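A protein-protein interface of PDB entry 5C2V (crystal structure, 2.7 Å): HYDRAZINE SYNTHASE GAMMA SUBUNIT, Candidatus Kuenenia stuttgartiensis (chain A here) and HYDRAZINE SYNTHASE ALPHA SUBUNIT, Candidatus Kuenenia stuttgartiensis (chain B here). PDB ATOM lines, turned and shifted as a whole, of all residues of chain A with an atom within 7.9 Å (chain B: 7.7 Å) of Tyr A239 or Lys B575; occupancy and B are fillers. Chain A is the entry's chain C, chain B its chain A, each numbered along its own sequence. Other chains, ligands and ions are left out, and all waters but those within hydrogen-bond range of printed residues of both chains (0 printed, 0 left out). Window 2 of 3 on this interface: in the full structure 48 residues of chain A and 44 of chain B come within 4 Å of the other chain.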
ATOM      1  N   TRP A  88     -27.387 -30.401  -3.157  1.00  0.00           N
ATOM      2  CA  TRP A  88     -26.215 -30.763  -3.950  1.00  0.00           C
ATOM      3  C   TRP A  88     -26.378 -32.068  -4.722  1.00  0.00           C
ATOM      4  O   TRP A  88     -26.999 -33.013  -4.234  1.00  0.00           O
ATOM      5  CB  TRP A  88     -24.986 -30.863  -3.043  1.00  0.00           C
ATOM      6  CG  TRP A  88     -24.714 -29.608  -2.281  1.00  0.00           C
ATOM      7  CD1 TRP A  88     -25.104 -29.319  -1.006  1.00  0.00           C
ATOM      8  CD2 TRP A  88     -23.998 -28.463  -2.752  1.00  0.00           C
ATOM      9  NE1 TRP A  88     -24.670 -28.065  -0.652  1.00  0.00           N
ATOM     10  CE2 TRP A  88     -23.989 -27.518  -1.706  1.00  0.00           C
ATOM     11  CE3 TRP A  88     -23.361 -28.146  -3.955  1.00  0.00           C
ATOM     12  CZ2 TRP A  88     -23.366 -26.278  -1.829  1.00  0.00           C
ATOM     13  CZ3 TRP A  88     -22.745 -26.914  -4.075  1.00  0.00           C
ATOM     14  CH2 TRP A  88     -22.752 -25.995  -3.018  1.00  0.00           C
ATOM     15  N   VAL A 216     -32.188 -28.258  10.171  1.00  0.00           N
ATOM     16  CA  VAL A 216     -32.080 -28.423  11.615  1.00  0.00           C
ATOM     17  C   VAL A 216     -33.458 -28.572  12.255  1.00  0.00           C
ATOM     18  O   VAL A 216     -33.598 -29.193  13.308  1.00  0.00           O
ATOM     19  CB  VAL A 216     -31.327 -27.239  12.264  1.00  0.00           C
ATOM     20  CG1 VAL A 216     -29.898 -27.173  11.746  1.00  0.00           C
ATOM     21  CG2 VAL A 216     -32.051 -25.925  11.999  1.00  0.00           C
ATOM     22  N   THR A 222     -34.616 -24.697   7.286  1.00  0.00           N
ATOM     23  CA  THR A 222     -33.298 -24.121   7.038  1.00  0.00           C
ATOM     24  C   THR A 222     -32.701 -23.616   8.355  1.00  0.00           C
ATOM     25  O   THR A 222     -33.438 -23.190   9.246  1.00  0.00           O
ATOM     26  CB  THR A 222     -33.385 -22.976   5.994  1.00  0.00           C
ATOM     27  OG1 THR A 222     -32.071 -22.548   5.614  1.00  0.00           O
ATOM     28  CG2 THR A 222     -34.170 -21.792   6.542  1.00  0.00           C
ATOM     29  N   PRO A 223     -31.364 -23.671   8.497  1.00  0.00           N
ATOM     30  CA  PRO A 223     -30.366 -24.196   7.560  1.00  0.00           C
ATOM     31  C   PRO A 223     -30.190 -25.707   7.656  1.00  0.00           C
ATOM     32  O   PRO A 223     -30.843 -26.358   8.471  1.00  0.00           O
ATOM     33  CB  PRO A 223     -29.088 -23.481   7.991  1.00  0.00           C
ATOM     34  CG  PRO A 223     -29.253 -23.340   9.463  1.00  0.00           C
ATOM     35  CD  PRO A 223     -30.727 -23.096   9.696  1.00  0.00           C
ATOM     36  N   GLY A 224     -29.302 -26.251   6.831  1.00  0.00           N
ATOM     37  CA  GLY A 224     -29.039 -27.676   6.826  1.00  0.00           C
ATOM     38  C   GLY A 224     -28.264 -28.126   8.046  1.00  0.00           C
ATOM     39  O   GLY A 224     -27.583 -27.331   8.693  1.00  0.00           O
ATOM     40  N   LYS A 225     -28.362 -29.414   8.352  1.00  0.00           N
ATOM     41  CA  LYS A 225     -27.655 -29.995   9.484  1.00  0.00           C
ATOM     42  C   LYS A 225     -26.550 -30.900   8.966  1.00  0.00           C
ATOM     43  O   LYS A 225     -26.636 -31.418   7.852  1.00  0.00           O
ATOM     44  CB  LYS A 225     -28.606 -30.782  10.390  1.00  0.00           C
ATOM     45  CG  LYS A 225     -29.045 -32.121   9.818  1.00  0.00           C
ATOM     46  CD  LYS A 225     -29.698 -32.994  10.878  1.00  0.00           C
ATOM     47  CE  LYS A 225     -30.942 -32.338  11.451  1.00  0.00           C
ATOM     48  NZ  LYS A 225     -31.617 -33.212  12.450  1.00  0.00           N
ATOM     49  N   VAL A 226     -25.503 -31.084   9.762  1.00  0.00           N
ATOM     50  CA  VAL A 226     -24.387 -31.901   9.319  1.00  0.00           C
ATOM     51  C   VAL A 226     -24.809 -33.364   9.332  1.00  0.00           C
ATOM     52  O   VAL A 226     -25.156 -33.911  10.379  1.00  0.00           O
ATOM     53  CB  VAL A 226     -23.151 -31.709  10.220  1.00  0.00           C
ATOM     54  CG1 VAL A 226     -21.981 -32.532   9.704  1.00  0.00           C
ATOM     55  CG2 VAL A 226     -22.782 -30.236  10.308  1.00  0.00           C
ATOM     56  N   GLU A 236     -15.116 -30.444  11.306  1.00  0.00           N
ATOM     57  CA  GLU A 236     -15.006 -29.852   9.979  1.00  0.00           C
ATOM     58  C   GLU A 236     -15.977 -28.683   9.819  1.00  0.00           C
ATOM     59  O   GLU A 236     -17.073 -28.695  10.379  1.00  0.00           O
ATOM     60  CB  GLU A 236     -15.264 -30.914   8.907  1.00  0.00           C
ATOM     61  CG  GLU A 236     -15.000 -30.458   7.481  1.00  0.00           C
ATOM     62  CD  GLU A 236     -15.129 -31.588   6.479  1.00  0.00           C
ATOM     63  OE1 GLU A 236     -15.178 -32.761   6.906  1.00  0.00           O
ATOM     64  OE2 GLU A 236     -15.185 -31.304   5.263  1.00  0.00           O
ATOM     65  N   ASP A 237     -15.563 -27.675   9.058  1.00  0.00           N
ATOM     66  CA  ASP A 237     -16.388 -26.496   8.819  1.00  0.00           C
ATOM     67  C   ASP A 237     -17.522 -26.818   7.849  1.00  0.00           C
ATOM     68  O   ASP A 237     -17.271 -27.203   6.707  1.00  0.00           O
ATOM     69  CB  ASP A 237     -15.529 -25.347   8.279  1.00  0.00           C
ATOM     70  CG  ASP A 237     -16.313 -24.059   8.096  1.00  0.00           C
ATOM     71  OD1 ASP A 237     -17.330 -23.869   8.794  1.00  0.00           O
ATOM     72  OD2 ASP A 237     -15.903 -23.226   7.262  1.00  0.00           O
ATOM     73  N   PRO A 238     -18.774 -26.670   8.310  1.00  0.00           N
ATOM     74  CA  PRO A 238     -19.961 -26.928   7.485  1.00  0.00           C
ATOM     75  C   PRO A 238     -19.946 -26.126   6.188  1.00  0.00           C
ATOM     76  O   PRO A 238     -20.259 -26.650   5.119  1.00  0.00           O
ATOM     77  CB  PRO A 238     -21.118 -26.482   8.386  1.00  0.00           C
ATOM     78  CG  PRO A 238     -20.590 -26.617   9.770  1.00  0.00           C
ATOM     79  CD  PRO A 238     -19.134 -26.274   9.683  1.00  0.00           C
ATOM     80  N   TYR A 239     -19.586 -24.853   6.300  1.00  0.00           N
ATOM     81  CA  TYR A 239     -19.547 -23.946   5.161  1.00  0.00           C
ATOM     82  C   TYR A 239     -18.148 -23.825   4.550  1.00  0.00           C
ATOM     83  O   TYR A 239     -17.911 -22.968   3.704  1.00  0.00           O
ATOM     84  CB  TYR A 239     -20.089 -22.578   5.575  1.00  0.00           C
ATOM     85  CG  TYR A 239     -21.544 -22.650   5.987  1.00  0.00           C
ATOM     86  CD1 TYR A 239     -22.553 -22.706   5.033  1.00  0.00           C
ATOM     87  CD2 TYR A 239     -21.907 -22.695   7.327  1.00  0.00           C
ATOM     88  CE1 TYR A 239     -23.883 -22.786   5.402  1.00  0.00           C
ATOM     89  CE2 TYR A 239     -23.237 -22.774   7.705  1.00  0.00           C
ATOM     90  CZ  TYR A 239     -24.219 -22.820   6.738  1.00  0.00           C
ATOM     91  OH  TYR A 239     -25.542 -22.898   7.105  1.00  0.00           O
ATOM     92  N   GLY A 240     -17.219 -24.658   5.014  1.00  0.00           N
ATOM     93  CA  GLY A 240     -15.865 -24.686   4.480  1.00  0.00           C
ATOM     94  C   GLY A 240     -15.780 -24.831   2.969  1.00  0.00           C
ATOM     95  O   GLY A 240     -16.553 -25.572   2.362  1.00  0.00           O
ATOM     96  N   VAL A 241     -14.841 -24.108   2.362  1.00  0.00           N
ATOM     97  CA  VAL A 241     -14.686 -24.095   0.909  1.00  0.00           C
ATOM     98  C   VAL A 241     -13.608 -25.064   0.403  1.00  0.00           C
ATOM     99  O   VAL A 241     -13.462 -25.267  -0.803  1.00  0.00           O
ATOM    100  CB  VAL A 241     -14.345 -22.663   0.418  1.00  0.00           C
ATOM    101  CG1 VAL A 241     -12.859 -22.381   0.590  1.00  0.00           C
ATOM    102  CG2 VAL A 241     -14.766 -22.461  -1.031  1.00  0.00           C
ATOM    103  N   GLU A 242     -12.867 -25.675   1.323  1.00  0.00           N
ATOM    104  CA  GLU A 242     -11.751 -26.543   0.944  1.00  0.00           C
ATOM    105  C   GLU A 242     -12.121 -28.023   0.854  1.00  0.00           C
ATOM    106  O   GLU A 242     -11.319 -28.840   0.400  1.00  0.00           O
ATOM    107  CB  GLU A 242     -10.592 -26.364   1.925  1.00  0.00           C
ATOM    108  CG  GLU A 242      -9.639 -25.237   1.557  1.00  0.00           C
ATOM    109  CD  GLU A 242      -8.738 -24.836   2.707  1.00  0.00           C
ATOM    110  OE1 GLU A 242      -9.246 -24.693   3.839  1.00  0.00           O
ATOM    111  OE2 GLU A 242      -7.521 -24.666   2.480  1.00  0.00           O
ATOM    112  N   SER A 243     -13.330 -28.364   1.284  1.00  0.00           N
ATOM    113  CA  SER A 243     -13.765 -29.757   1.315  1.00  0.00           C
ATOM    114  C   SER A 243     -14.049 -30.290  -0.084  1.00  0.00           C
ATOM    115  O   SER A 243     -14.570 -29.571  -0.932  1.00  0.00           O
ATOM    116  CB  SER A 243     -15.011 -29.907   2.188  1.00  0.00           C
ATOM    117  OG  SER A 243     -14.792 -29.377   3.483  1.00  0.00           O
ATOM    118  N   ILE A 247     -20.678 -31.498   3.657  1.00  0.00           N
ATOM    119  CA  ILE A 247     -21.168 -32.245   4.809  1.00  0.00           C
ATOM    120  C   ILE A 247     -22.554 -31.759   5.242  1.00  0.00           C
ATOM    121  O   ILE A 247     -23.103 -32.234   6.236  1.00  0.00           O
ATOM    122  CB  ILE A 247     -20.193 -32.166   6.001  1.00  0.00           C
ATOM    123  CG1 ILE A 247     -19.893 -30.711   6.368  1.00  0.00           C
ATOM    124  CG2 ILE A 247     -18.904 -32.910   5.681  1.00  0.00           C
ATOM    125  CD1 ILE A 247     -18.864 -30.569   7.473  1.00  0.00           C
ATOM    126  N   ILE A 248     -23.111 -30.809   4.493  1.00  0.00           N
ATOM    127  CA  ILE A 248     -24.464 -30.312   4.746  1.00  0.00           C
ATOM    128  C   ILE A 248     -25.281 -30.258   3.458  1.00  0.00           C
ATOM    129  O   ILE A 248     -24.737 -30.408   2.364  1.00  0.00           O
ATOM    130  CB  ILE A 248     -24.460 -28.902   5.377  1.00  0.00           C
ATOM    131  CG1 ILE A 248     -23.905 -27.874   4.388  1.00  0.00           C
ATOM    132  CG2 ILE A 248     -23.675 -28.891   6.682  1.00  0.00           C
ATOM    133  CD1 ILE A 248     -23.944 -26.451   4.902  1.00  0.00           C
ATOM    134  N   LEU A 250     -29.724 -29.314   1.835  1.00  0.00           N
ATOM    135  CA  LEU A 250     -31.174 -29.313   1.969  1.00  0.00           C
ATOM    136  C   LEU A 250     -31.808 -29.946   0.739  1.00  0.00           C
ATOM    137  O   LEU A 250     -31.787 -29.363  -0.340  1.00  0.00           O
ATOM    138  CB  LEU A 250     -31.704 -27.891   2.159  1.00  0.00           C
ATOM    139  CG  LEU A 250     -31.263 -27.149   3.418  1.00  0.00           C
ATOM    140  CD1 LEU A 250     -31.697 -25.692   3.372  1.00  0.00           C
ATOM    141  CD2 LEU A 250     -31.838 -27.841   4.634  1.00  0.00           C
ATOM    142  N   ILE B 432     -28.902 -12.231  -4.617  1.00  0.00           N
ATOM    143  CA  ILE B 432     -27.987 -12.733  -3.602  1.00  0.00           C
ATOM    144  C   ILE B 432     -26.539 -12.293  -3.849  1.00  0.00           C
ATOM    145  O   ILE B 432     -26.006 -12.396  -4.964  1.00  0.00           O
ATOM    146  CB  ILE B 432     -28.057 -14.280  -3.515  1.00  0.00           C
ATOM    147  CG1 ILE B 432     -27.014 -14.820  -2.535  1.00  0.00           C
ATOM    148  CG2 ILE B 432     -27.888 -14.912  -4.890  1.00  0.00           C
ATOM    149  CD1 ILE B 432     -27.070 -16.320  -2.350  1.00  0.00           C
ATOM    150  N   CYS B 433     -25.919 -11.781  -2.791  1.00  0.00           N
ATOM    151  CA  CYS B 433     -24.508 -11.428  -2.802  1.00  0.00           C
ATOM    152  C   CYS B 433     -23.762 -12.348  -1.845  1.00  0.00           C
ATOM    153  O   CYS B 433     -24.143 -12.481  -0.684  1.00  0.00           O
ATOM    154  CB  CYS B 433     -24.304  -9.964  -2.409  1.00  0.00           C
ATOM    155  SG  CYS B 433     -22.578  -9.421  -2.427  1.00  0.00           S
ATOM    156  N   PHE B 434     -22.702 -12.980  -2.335  1.00  0.00           N
ATOM    157  CA  PHE B 434     -21.997 -13.987  -1.553  1.00  0.00           C
ATOM    158  C   PHE B 434     -21.080 -13.365  -0.500  1.00  0.00           C
ATOM    159  O   PHE B 434     -20.924 -13.914   0.590  1.00  0.00           O
ATOM    160  CB  PHE B 434     -21.211 -14.912  -2.485  1.00  0.00           C
ATOM    161  CG  PHE B 434     -22.083 -15.656  -3.461  1.00  0.00           C
ATOM    162  CD1 PHE B 434     -22.776 -16.791  -3.069  1.00  0.00           C
ATOM    163  CD2 PHE B 434     -22.226 -15.210  -4.764  1.00  0.00           C
ATOM    164  CE1 PHE B 434     -23.584 -17.471  -3.962  1.00  0.00           C
ATOM    165  CE2 PHE B 434     -23.034 -15.885  -5.661  1.00  0.00           C
ATOM    166  CZ  PHE B 434     -23.713 -17.017  -5.259  1.00  0.00           C
ATOM    167  N   GLU B 512     -25.681 -12.287   6.778  1.00  0.00           N
ATOM    168  CA  GLU B 512     -25.096 -13.382   7.543  1.00  0.00           C
ATOM    169  C   GLU B 512     -23.688 -13.039   8.023  1.00  0.00           C
ATOM    170  O   GLU B 512     -23.043 -12.133   7.494  1.00  0.00           O
ATOM    171  CB  GLU B 512     -25.070 -14.665   6.707  1.00  0.00           C
ATOM    172  CG  GLU B 512     -26.417 -15.064   6.115  1.00  0.00           C
ATOM    173  CD  GLU B 512     -27.327 -15.763   7.112  1.00  0.00           C
ATOM    174  OE1 GLU B 512     -27.068 -15.682   8.331  1.00  0.00           O
ATOM    175  OE2 GLU B 512     -28.305 -16.402   6.670  1.00  0.00           O
ATOM    176  N   SER B 513     -23.222 -13.768   9.033  1.00  0.00           N
ATOM    177  CA  SER B 513     -21.921 -13.508   9.647  1.00  0.00           C
ATOM    178  C   SER B 513     -20.750 -13.697   8.682  1.00  0.00           C
ATOM    179  O   SER B 513     -19.633 -13.262   8.964  1.00  0.00           O
ATOM    180  CB  SER B 513     -21.730 -14.406  10.872  1.00  0.00           C
ATOM    181  OG  SER B 513     -21.638 -15.772  10.499  1.00  0.00           O
ATOM    182  N   ASP B 514     -21.000 -14.349   7.551  1.00  0.00           N
ATOM    183  CA  ASP B 514     -19.964 -14.533   6.538  1.00  0.00           C
ATOM    184  C   ASP B 514     -20.041 -13.443   5.470  1.00  0.00           C
ATOM    185  O   ASP B 514     -19.281 -13.455   4.502  1.00  0.00           O
ATOM    186  CB  ASP B 514     -20.069 -15.921   5.899  1.00  0.00           C
ATOM    187  CG  ASP B 514     -21.353 -16.112   5.114  1.00  0.00           C
ATOM    188  OD1 ASP B 514     -22.324 -15.370   5.362  1.00  0.00           O
ATOM    189  OD2 ASP B 514     -21.391 -17.013   4.250  1.00  0.00           O
ATOM    190  N   GLY B 515     -20.968 -12.506   5.650  1.00  0.00           N
ATOM    191  CA  GLY B 515     -21.093 -11.369   4.756  1.00  0.00           C
ATOM    192  C   GLY B 515     -22.096 -11.571   3.637  1.00  0.00           C
ATOM    193  O   GLY B 515     -22.430 -10.630   2.917  1.00  0.00           O
ATOM    194  N   SER B 516     -22.580 -12.799   3.493  1.00  0.00           N
ATOM    195  CA  SER B 516     -23.534 -13.126   2.440  1.00  0.00           C
ATOM    196  C   SER B 516     -24.942 -12.649   2.779  1.00  0.00           C
ATOM    197  O   SER B 516     -25.312 -12.552   3.949  1.00  0.00           O
ATOM    198  CB  SER B 516     -23.548 -14.632   2.180  1.00  0.00           C
ATOM    199  OG  SER B 516     -23.882 -15.349   3.356  1.00  0.00           O
ATOM    200  N   THR B 517     -25.720 -12.347   1.745  1.00  0.00           N
ATOM    201  CA  THR B 517     -27.114 -11.963   1.926  1.00  0.00           C
ATOM    202  C   THR B 517     -27.949 -12.354   0.710  1.00  0.00           C
ATOM    203  O   THR B 517     -27.443 -12.424  -0.411  1.00  0.00           O
ATOM    204  CB  THR B 517     -27.263 -10.449   2.179  1.00  0.00           C
ATOM    205  OG1 THR B 517     -28.638 -10.139   2.440  1.00  0.00           O
ATOM    206  CG2 THR B 517     -26.787  -9.650   0.974  1.00  0.00           C
ATOM    207  N   VAL B 518     -29.229 -12.619   0.944  1.00  0.00           N
ATOM    208  CA  VAL B 518     -30.161 -12.936  -0.130  1.00  0.00           C
ATOM    209  C   VAL B 518     -31.527 -12.361   0.224  1.00  0.00           C
ATOM    210  O   VAL B 518     -31.918 -12.356   1.392  1.00  0.00           O
ATOM    211  CB  VAL B 518     -30.264 -14.463  -0.373  1.00  0.00           C
ATOM    212  CG1 VAL B 518     -30.722 -15.183   0.887  1.00  0.00           C
ATOM    213  CG2 VAL B 518     -31.195 -14.768  -1.542  1.00  0.00           C
ATOM    214  N   ILE B 572     -17.085 -19.416  -3.361  1.00  0.00           N
ATOM    215  CA  ILE B 572     -17.505 -19.057  -2.016  1.00  0.00           C
ATOM    216  C   ILE B 572     -18.632 -19.969  -1.570  1.00  0.00           C
ATOM    217  O   ILE B 572     -19.605 -20.173  -2.296  1.00  0.00           O
ATOM    218  CB  ILE B 572     -17.986 -17.586  -1.927  1.00  0.00           C
ATOM    219  CG1 ILE B 572     -16.904 -16.618  -2.415  1.00  0.00           C
ATOM    220  CG2 ILE B 572     -18.398 -17.239  -0.504  1.00  0.00           C
ATOM    221  CD1 ILE B 572     -17.299 -15.160  -2.314  1.00  0.00           C
ATOM    222  N   HIS B 573     -18.500 -20.515  -0.370  1.00  0.00           N
ATOM    223  CA  HIS B 573     -19.558 -21.323   0.205  1.00  0.00           C
ATOM    224  C   HIS B 573     -20.296 -20.446   1.206  1.00  0.00           C
ATOM    225  O   HIS B 573     -19.785 -20.155   2.287  1.00  0.00           O
ATOM    226  CB  HIS B 573     -18.975 -22.572   0.864  1.00  0.00           C
ATOM    227  CG  HIS B 573     -19.987 -23.628   1.177  1.00  0.00           C
ATOM    228  ND1 HIS B 573     -19.650 -24.823   1.776  1.00  0.00           N
ATOM    229  CD2 HIS B 573     -21.324 -23.677   0.971  1.00  0.00           C
ATOM    230  CE1 HIS B 573     -20.735 -25.559   1.928  1.00  0.00           C
ATOM    231  NE2 HIS B 573     -21.765 -24.887   1.447  1.00  0.00           N
ATOM    232  N   ALA B 574     -21.505 -20.033   0.842  1.00  0.00           N
ATOM    233  CA  ALA B 574     -22.196 -18.980   1.576  1.00  0.00           C
ATOM    234  C   ALA B 574     -23.440 -19.487   2.289  1.00  0.00           C
ATOM    235  O   ALA B 574     -24.140 -20.368   1.790  1.00  0.00           O
ATOM    236  CB  ALA B 574     -22.559 -17.842   0.634  1.00  0.00           C
ATOM    237  N   LYS B 575     -23.709 -18.919   3.459  1.00  0.00           N
ATOM    238  CA  LYS B 575     -24.875 -19.294   4.246  1.00  0.00           C
ATOM    239  C   LYS B 575     -26.170 -18.910   3.540  1.00  0.00           C
ATOM    240  O   LYS B 575     -27.177 -19.608   3.649  1.00  0.00           O
ATOM    241  CB  LYS B 575     -24.825 -18.639   5.627  1.00  0.00           C
ATOM    242  CG  LYS B 575     -23.673 -19.098   6.503  1.00  0.00           C
ATOM    243  CD  LYS B 575     -23.808 -18.533   7.908  1.00  0.00           C
ATOM    244  CE  LYS B 575     -22.694 -19.020   8.817  1.00  0.00           C
ATOM    245  NZ  LYS B 575     -22.868 -18.519  10.210  1.00  0.00           N
ATOM    246  N   ALA B 576     -26.132 -17.797   2.815  1.00  0.00           N
ATOM    247  CA  ALA B 576     -27.311 -17.272   2.135  1.00  0.00           C
ATOM    248  C   ALA B 576     -27.838 -18.239   1.079  1.00  0.00           C
ATOM    249  O   ALA B 576     -29.033 -18.250   0.780  1.00  0.00           O
ATOM    250  CB  ALA B 576     -26.997 -15.926   1.505  1.00  0.00           C
ATOM    251  N   LEU B 577     -26.939 -19.047   0.521  1.00  0.00           N
ATOM    252  CA  LEU B 577     -27.298 -20.034  -0.492  1.00  0.00           C
ATOM    253  C   LEU B 577     -28.389 -20.981  -0.001  1.00  0.00           C
ATOM    254  O   LEU B 577     -29.258 -21.399  -0.768  1.00  0.00           O
ATOM    255  CB  LEU B 577     -26.065 -20.836  -0.912  1.00  0.00           C
ATOM    256  CG  LEU B 577     -26.315 -22.020  -1.848  1.00  0.00           C
ATOM    257  CD1 LEU B 577     -26.937 -21.546  -3.150  1.00  0.00           C
ATOM    258  CD2 LEU B 577     -25.032 -22.794  -2.110  1.00  0.00           C
ATOM    259  N   TYR B 578     -28.343 -21.310   1.284  1.00  0.00           N
ATOM    260  CA  TYR B 578     -29.294 -22.244   1.870  1.00  0.00           C
ATOM    261  C   TYR B 578     -30.567 -21.538   2.326  1.00  0.00           C
ATOM    262  O   TYR B 578     -31.548 -22.184   2.690  1.00  0.00           O
ATOM    263  CB  TYR B 578     -28.647 -22.990   3.037  1.00  0.00           C
ATOM    264  CG  TYR B 578     -27.462 -23.834   2.620  1.00  0.00           C
ATOM    265  CD1 TYR B 578     -27.634 -25.145   2.197  1.00  0.00           C
ATOM    266  CD2 TYR B 578     -26.173 -23.315   2.639  1.00  0.00           C
ATOM    267  CE1 TYR B 578     -26.556 -25.919   1.809  1.00  0.00           C
ATOM    268  CE2 TYR B 578     -25.088 -24.082   2.253  1.00  0.00           C
ATOM    269  CZ  TYR B 578     -25.286 -25.383   1.839  1.00  0.00           C
ATOM    270  OH  TYR B 578     -24.211 -26.151   1.453  1.00  0.00           O
ATOM    271  N   ASN B 579     -30.549 -20.209   2.304  1.00  0.00           N
ATOM    272  CA  ASN B 579     -31.728 -19.425   2.651  1.00  0.00           C
ATOM    273  C   ASN B 579     -32.528 -19.027   1.412  1.00  0.00           C
ATOM    274  O   ASN B 579     -33.494 -18.269   1.506  1.00  0.00           O
ATOM    275  CB  ASN B 579     -31.332 -18.177   3.442  1.00  0.00           C
ATOM    276  CG  ASN B 579     -32.454 -17.668   4.332  1.00  0.00           C
ATOM    277  OD1 ASN B 579     -33.355 -18.421   4.701  1.00  0.00           O
ATOM    278  ND2 ASN B 579     -32.400 -16.387   4.685  1.00  0.00           N
ATOM    279  N   TRP B 580     -32.123 -19.536   0.251  1.00  0.00           N
ATOM    280  CA  TRP B 580     -32.703 -19.090  -1.013  1.00  0.00           C
ATOM    281  C   TRP B 580     -33.957 -19.877  -1.415  1.00  0.00           C
ATOM    282  O   TRP B 580     -35.071 -19.369  -1.289  1.00  0.00           O
ATOM    283  CB  TRP B 580     -31.650 -19.187  -2.117  1.00  0.00           C
ATOM    284  CG  TRP B 580     -31.886 -18.278  -3.279  1.00  0.00           C
ATOM    285  CD1 TRP B 580     -32.919 -17.400  -3.443  1.00  0.00           C
ATOM    286  CD2 TRP B 580     -31.054 -18.140  -4.437  1.00  0.00           C
ATOM    287  NE1 TRP B 580     -32.787 -16.733  -4.638  1.00  0.00           N
ATOM    288  CE2 TRP B 580     -31.650 -17.169  -5.266  1.00  0.00           C
ATOM    289  CE3 TRP B 580     -29.867 -18.747  -4.855  1.00  0.00           C
ATOM    290  CZ2 TRP B 580     -31.097 -16.793  -6.488  1.00  0.00           C
ATOM    291  CZ3 TRP B 580     -29.322 -18.375  -6.068  1.00  0.00           C
ATOM    292  CH2 TRP B 580     -29.936 -17.406  -6.869  1.00  0.00           C
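NE2 of His B573 touches CZ2 of Trp A88 (3.9 Å).
Leu B577 touches Trp A88 (CD2 to CZ2, 3.9 Å).
Thr A222 touches Asn B579.
CE1 of His B573 touches O of Pro A238 (3.4 Å).
Lys B575 touches Tyr A239.
Tyr A239 touches Tyr B578.
CG1 of Ile A248 touches OH of Tyr B578, 3.4 Å away.
Tyr B578 touches Leu A250.
Of chain B, only His B573 (3.1 Å), Lys B575 (3.8 Å) and Tyr B578 (3.6 Å) come within 4 Å of Tyr A239.
Ala B576 touches none of the printed residues of chain A.
Of the printed residues of chain A, Leu B577 touches Trp A88 (3.9 Å).
Of the printed residues of chain A, His B573 touches Trp A88, Pro A238, Tyr A239 and Gly A240.
Printed residues of chain B within 4 Å of Thr A222: Tyr B578 and Asn B579.
Printed residues of chain A within 4 Å of Tyr B578: Trp A88, Thr A222, Tyr A239, Ile A248 and Leu A250.
Lys A225 touches none of the printed residues of chain B.
Glu A236 touches none of the printed residues of chain B.
The nearest residue of chain B that does not touch Tyr A239 is Ala B574 (4.3 Å).
The nearest residue of chain A that does not touch Lys B575 is Thr A222 (6.0 Å).
Of the 18 printed residues of chain A, 7 touch a printed residue of chain B.
Hydrophobic or aromatic side chains of chain B that line the printed part of chain A: His B573, Leu B577 and Tyr B578.
Among the printed residues, 12 pairs touch across the chains.
ND1 of His B573 is in hydrogen-bond range of O of Gly A240, 3.2 Å away.
NE1 of Trp A88 is in hydrogen-bond range of OH of Tyr B578 (2.9 Å).
The backbone carbonyl oxygen (O) of Tyr A239 sits close to a ring nitrogen (ND1) of His B573.
The side-chain hydroxyl (OG1) of Thr A222 is in hydrogen-bond range of the backbone carbonyl oxygen (O) of Tyr B578 (3.0 Å).
The backbone NH (N) of Lys B575 is in hydrogen-bond range of the side-chain carboxylate (OD2) of Asp B514, 3.1 Å away.
The backbone NH (N) of Gly A240 is in hydrogen-bond range of the side-chain carboxylate (OD2) of Asp A237 (3.0 Å).
The side-chain hydroxyl of Ser B513 lies within hydrogen-bond range of the side-chain amino group of Lys B575, 3.0 Å away.
NE2 of His B573 sits at hydrogen-bond distance from OH of Tyr B578, 2.8 Å away.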
